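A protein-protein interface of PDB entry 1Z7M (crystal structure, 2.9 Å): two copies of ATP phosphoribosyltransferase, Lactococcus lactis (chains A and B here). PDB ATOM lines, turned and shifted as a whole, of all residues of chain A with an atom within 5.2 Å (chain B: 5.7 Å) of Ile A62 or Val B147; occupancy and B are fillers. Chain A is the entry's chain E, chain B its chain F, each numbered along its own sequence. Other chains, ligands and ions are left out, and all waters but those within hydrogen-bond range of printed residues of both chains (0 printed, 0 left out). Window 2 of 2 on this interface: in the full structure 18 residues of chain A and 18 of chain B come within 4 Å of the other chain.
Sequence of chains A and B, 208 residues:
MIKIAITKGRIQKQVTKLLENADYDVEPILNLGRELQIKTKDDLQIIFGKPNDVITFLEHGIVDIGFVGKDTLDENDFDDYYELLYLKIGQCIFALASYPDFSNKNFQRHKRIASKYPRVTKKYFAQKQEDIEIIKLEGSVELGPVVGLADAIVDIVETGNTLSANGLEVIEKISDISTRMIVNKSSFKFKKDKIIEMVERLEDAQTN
The backbone carbonyl oxygen (O) of Phe A57 lies within hydrogen-bond range of the backbone NH (N) of Ile A62, at 2.9 Å. The backbone carbonyl oxygen (O) of Gly B144 sits at hydrogen-bond distance from the backbone NH (N) of Leu B149 (2.9 Å).
Among the printed residues, pairs that only touch across the chains: Phe A57 with Leu B149 (3.1 Å), Gln A37 with Val B146 (3.5 Å), His A60 with Leu B149 (3.5 Å), Gln A37 with Val B147 (3.5 Å), Ile A47 with Val B147 (3.5 Å), Ile A62 with Val B147 (3.6 Å), Ile A47 with Leu B143 (3.6 Å) and Ile A62 with Leu B149 (3.7 Å).
Lys A3 touches none of the printed residues of chain B. Of the printed residues of chain B, Phe A57 touches Leu B149 (3.1 Å). Ile A62 touches just these residues of chain B: Val B147 and Leu B149. Val B147 touches just these residues of chain A: Gln A37, Ile A47 and Ile A62. Printed residues of chain A within 4 Å of Leu B149: Phe A57 (3.1 Å), His A60 (3.5 Å) and Ile A62 (3.7 Å). The nearest printed residue of chain A that does not touch Leu B143 is Phe A57 (4.4 Å).
Printed residues of chain B that touch a printed residue of chain A: Leu B143, Val B146, Val B147 and Leu B149. Along chain A the printed residues that touch a printed residue of chain B span positions 37 to 62.
No position is printed for both chains. Of the 8 pairs that touch across the chains among the printed residues, none has its exchanged pair printed and touching as well.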
ATOM      1  N   LYS A   3     -26.663 -15.717   8.867  1.00  0.00           N
ATOM      2  CA  LYS A   3     -25.204 -15.762   9.011  1.00  0.00           C
ATOM      3  C   LYS A   3     -24.736 -16.421  10.312  1.00  0.00           C
ATOM      4  O   LYS A   3     -25.207 -16.085  11.391  1.00  0.00           O
ATOM      5  CB  LYS A   3     -24.646 -14.343   8.920  1.00  0.00           C
ATOM      6  CG  LYS A   3     -25.248 -13.522   7.798  1.00  0.00           C
ATOM      7  CD  LYS A   3     -24.455 -12.256   7.596  1.00  0.00           C
ATOM      8  CE  LYS A   3     -24.951 -11.491   6.392  1.00  0.00           C
ATOM      9  NZ  LYS A   3     -24.110 -10.289   6.092  1.00  0.00           N
ATOM     10  N   GLN A  37     -15.502 -17.752   4.437  1.00  0.00           N
ATOM     11  CA  GLN A  37     -16.938 -17.461   4.390  1.00  0.00           C
ATOM     12  C   GLN A  37     -17.620 -18.149   3.213  1.00  0.00           C
ATOM     13  O   GLN A  37     -17.517 -17.700   2.073  1.00  0.00           O
ATOM     14  CB  GLN A  37     -17.202 -15.953   4.316  1.00  0.00           C
ATOM     15  CG  GLN A  37     -16.435 -15.213   3.226  1.00  0.00           C
ATOM     16  CD  GLN A  37     -16.936 -13.785   3.010  1.00  0.00           C
ATOM     17  OE1 GLN A  37     -17.190 -13.043   3.969  1.00  0.00           O
ATOM     18  NE2 GLN A  37     -17.060 -13.387   1.744  1.00  0.00           N
ATOM     19  N   ILE A  47     -18.970 -18.618   8.688  1.00  0.00           N
ATOM     20  CA  ILE A  47     -17.616 -18.057   8.817  1.00  0.00           C
ATOM     21  C   ILE A  47     -16.907 -18.868   9.897  1.00  0.00           C
ATOM     22  O   ILE A  47     -17.562 -19.445  10.771  1.00  0.00           O
ATOM     23  CB  ILE A  47     -17.625 -16.570   9.282  1.00  0.00           C
ATOM     24  CG1 ILE A  47     -18.265 -15.677   8.219  1.00  0.00           C
ATOM     25  CG2 ILE A  47     -16.212 -16.096   9.534  1.00  0.00           C
ATOM     26  CD1 ILE A  47     -18.249 -14.196   8.583  1.00  0.00           C
ATOM     27  N   PHE A  57     -17.260 -11.448  16.331  1.00  0.00           N
ATOM     28  CA  PHE A  57     -18.103 -11.356  15.133  1.00  0.00           C
ATOM     29  C   PHE A  57     -19.570 -11.279  15.477  1.00  0.00           C
ATOM     30  O   PHE A  57     -20.311 -10.496  14.888  1.00  0.00           O
ATOM     31  CB  PHE A  57     -17.884 -12.553  14.213  1.00  0.00           C
ATOM     32  CG  PHE A  57     -16.621 -12.486  13.442  1.00  0.00           C
ATOM     33  CD1 PHE A  57     -15.892 -13.639  13.190  1.00  0.00           C
ATOM     34  CD2 PHE A  57     -16.134 -11.266  12.999  1.00  0.00           C
ATOM     35  CE1 PHE A  57     -14.686 -13.582  12.514  1.00  0.00           C
ATOM     36  CE2 PHE A  57     -14.932 -11.195  12.323  1.00  0.00           C
ATOM     37  CZ  PHE A  57     -14.203 -12.359  12.082  1.00  0.00           C
ATOM     38  N   LEU A  58     -19.992 -12.112  16.418  1.00  0.00           N
ATOM     39  CA  LEU A  58     -21.379 -12.117  16.834  1.00  0.00           C
ATOM     40  C   LEU A  58     -21.728 -10.807  17.528  1.00  0.00           C
ATOM     41  O   LEU A  58     -22.868 -10.346  17.475  1.00  0.00           O
ATOM     42  CB  LEU A  58     -21.651 -13.287  17.772  1.00  0.00           C
ATOM     43  CG  LEU A  58     -23.056 -13.201  18.361  1.00  0.00           C
ATOM     44  CD1 LEU A  58     -23.736 -14.566  18.331  1.00  0.00           C
ATOM     45  CD2 LEU A  58     -22.958 -12.634  19.765  1.00  0.00           C
ATOM     46  N   HIS A  60     -20.301  -7.680  16.908  1.00  0.00           N
ATOM     47  CA  HIS A  60     -20.461  -6.624  15.917  1.00  0.00           C
ATOM     48  C   HIS A  60     -21.544  -6.887  14.872  1.00  0.00           C
ATOM     49  O   HIS A  60     -21.586  -6.245  13.822  1.00  0.00           O
ATOM     50  CB  HIS A  60     -19.127  -6.340  15.237  1.00  0.00           C
ATOM     51  CG  HIS A  60     -18.149  -5.621  16.113  1.00  0.00           C
ATOM     52  ND1 HIS A  60     -17.550  -6.216  17.205  1.00  0.00           N
ATOM     53  CD2 HIS A  60     -17.671  -4.354  16.065  1.00  0.00           C
ATOM     54  CE1 HIS A  60     -16.742  -5.347  17.789  1.00  0.00           C
ATOM     55  NE2 HIS A  60     -16.796  -4.210  17.119  1.00  0.00           N
ATOM     56  N   GLY A  61     -22.429  -7.830  15.169  1.00  0.00           N
ATOM     57  CA  GLY A  61     -23.511  -8.133  14.251  1.00  0.00           C
ATOM     58  C   GLY A  61     -23.082  -8.663  12.900  1.00  0.00           C
ATOM     59  O   GLY A  61     -23.870  -8.651  11.955  1.00  0.00           O
ATOM     60  N   ILE A  62     -21.835  -9.121  12.799  1.00  0.00           N
ATOM     61  CA  ILE A  62     -21.312  -9.677  11.551  1.00  0.00           C
ATOM     62  C   ILE A  62     -22.061 -10.976  11.279  1.00  0.00           C
ATOM     63  O   ILE A  62     -22.184 -11.427  10.142  1.00  0.00           O
ATOM     64  CB  ILE A  62     -19.804  -9.973  11.664  1.00  0.00           C
ATOM     65  CG1 ILE A  62     -19.027  -8.669  11.873  1.00  0.00           C
ATOM     66  CG2 ILE A  62     -19.326 -10.719  10.439  1.00  0.00           C
ATOM     67  CD1 ILE A  62     -19.338  -7.587  10.869  1.00  0.00           C
ATOM     68  N   VAL A  63     -22.567 -11.575  12.344  1.00  0.00           N
ATOM     69  CA  VAL A  63     -23.328 -12.799  12.218  1.00  0.00           C
ATOM     70  C   VAL A  63     -24.508 -12.786  13.195  1.00  0.00           C
ATOM     71  O   VAL A  63     -24.609 -11.908  14.049  1.00  0.00           O
ATOM     72  CB  VAL A  63     -22.430 -14.033  12.464  1.00  0.00           C
ATOM     73  CG1 VAL A  63     -21.317 -14.045  11.469  1.00  0.00           C
ATOM     74  CG2 VAL A  63     -21.869 -14.014  13.868  1.00  0.00           C
ATOM     75  N   ASP A  64     -25.400 -13.760  13.048  1.00  0.00           N
ATOM     76  CA  ASP A  64     -26.573 -13.884  13.901  1.00  0.00           C
ATOM     77  C   ASP A  64     -26.327 -14.934  14.964  1.00  0.00           C
ATOM     78  O   ASP A  64     -26.479 -14.694  16.161  1.00  0.00           O
ATOM     79  CB  ASP A  64     -27.771 -14.300  13.064  1.00  0.00           C
ATOM     80  CG  ASP A  64     -27.972 -13.398  11.892  1.00  0.00           C
ATOM     81  OD1 ASP A  64     -27.353 -13.625  10.828  1.00  0.00           O
ATOM     82  OD2 ASP A  64     -28.743 -12.434  12.046  1.00  0.00           O
ATOM     83  N   LEU B 143     -10.183 -11.262   7.360  1.00  0.00           N
ATOM     84  CA  LEU B 143     -11.645 -11.123   7.346  1.00  0.00           C
ATOM     85  C   LEU B 143     -12.127  -9.798   7.894  1.00  0.00           C
ATOM     86  O   LEU B 143     -13.266  -9.416   7.656  1.00  0.00           O
ATOM     87  CB  LEU B 143     -12.326 -12.242   8.143  1.00  0.00           C
ATOM     88  CG  LEU B 143     -12.255 -13.668   7.606  1.00  0.00           C
ATOM     89  CD1 LEU B 143     -10.816 -14.149   7.687  1.00  0.00           C
ATOM     90  CD2 LEU B 143     -13.172 -14.578   8.420  1.00  0.00           C
ATOM     91  N   GLY B 144     -11.265  -9.107   8.632  1.00  0.00           N
ATOM     92  CA  GLY B 144     -11.635  -7.826   9.209  1.00  0.00           C
ATOM     93  C   GLY B 144     -12.364  -6.943   8.220  1.00  0.00           C
ATOM     94  O   GLY B 144     -13.505  -6.535   8.455  1.00  0.00           O
ATOM     95  N   PRO B 145     -11.718  -6.613   7.099  1.00  0.00           N
ATOM     96  CA  PRO B 145     -12.340  -5.767   6.078  1.00  0.00           C
ATOM     97  C   PRO B 145     -13.282  -6.566   5.173  1.00  0.00           C
ATOM     98  O   PRO B 145     -14.259  -6.032   4.652  1.00  0.00           O
ATOM     99  CB  PRO B 145     -11.137  -5.200   5.337  1.00  0.00           C
ATOM    100  CG  PRO B 145     -10.139  -6.323   5.433  1.00  0.00           C
ATOM    101  CD  PRO B 145     -10.271  -6.765   6.861  1.00  0.00           C
ATOM    102  N   VAL B 146     -12.981  -7.850   5.002  1.00  0.00           N
ATOM    103  CA  VAL B 146     -13.798  -8.732   4.177  1.00  0.00           C
ATOM    104  C   VAL B 146     -15.265  -8.709   4.581  1.00  0.00           C
ATOM    105  O   VAL B 146     -16.130  -8.407   3.761  1.00  0.00           O
ATOM    106  CB  VAL B 146     -13.313 -10.180   4.264  1.00  0.00           C
ATOM    107  CG1 VAL B 146     -14.334 -11.115   3.628  1.00  0.00           C
ATOM    108  CG2 VAL B 146     -11.970 -10.300   3.583  1.00  0.00           C
ATOM    109  N   VAL B 147     -15.549  -9.044   5.838  1.00  0.00           N
ATOM    110  CA  VAL B 147     -16.928  -9.052   6.323  1.00  0.00           C
ATOM    111  C   VAL B 147     -17.360  -7.656   6.775  1.00  0.00           C
ATOM    112  O   VAL B 147     -18.374  -7.496   7.445  1.00  0.00           O
ATOM    113  CB  VAL B 147     -17.114 -10.058   7.488  1.00  0.00           C
ATOM    114  CG1 VAL B 147     -16.625 -11.446   7.068  1.00  0.00           C
ATOM    115  CG2 VAL B 147     -16.369  -9.581   8.716  1.00  0.00           C
ATOM    116  N   GLY B 148     -16.584  -6.647   6.387  1.00  0.00           N
ATOM    117  CA  GLY B 148     -16.910  -5.277   6.738  1.00  0.00           C
ATOM    118  C   GLY B 148     -16.694  -4.923   8.193  1.00  0.00           C
ATOM    119  O   GLY B 148     -16.898  -3.774   8.589  1.00  0.00           O
ATOM    120  N   LEU B 149     -16.273  -5.912   8.980  1.00  0.00           N
ATOM    121  CA  LEU B 149     -16.029  -5.751  10.415  1.00  0.00           C
ATOM    122  C   LEU B 149     -15.075  -4.614  10.774  1.00  0.00           C
ATOM    123  O   LEU B 149     -15.156  -4.045  11.871  1.00  0.00           O
ATOM    124  CB  LEU B 149     -15.477  -7.052  10.996  1.00  0.00           C
ATOM    125  CG  LEU B 149     -15.035  -6.939  12.455  1.00  0.00           C
ATOM    126  CD1 LEU B 149     -16.269  -6.748  13.320  1.00  0.00           C
ATOM    127  CD2 LEU B 149     -14.248  -8.183  12.878  1.00  0.00           C
ATOM    128  N   ALA B 150     -14.167  -4.315   9.848  1.00  0.00           N
ATOM    129  CA  ALA B 150     -13.166  -3.260  10.009  1.00  0.00           C
ATOM    130  C   ALA B 150     -12.732  -2.779   8.642  1.00  0.00           C
ATOM    131  O   ALA B 150     -12.947  -3.456   7.642  1.00  0.00           O
ATOM    132  CB  ALA B 150     -11.961  -3.787  10.755  1.00  0.00           C
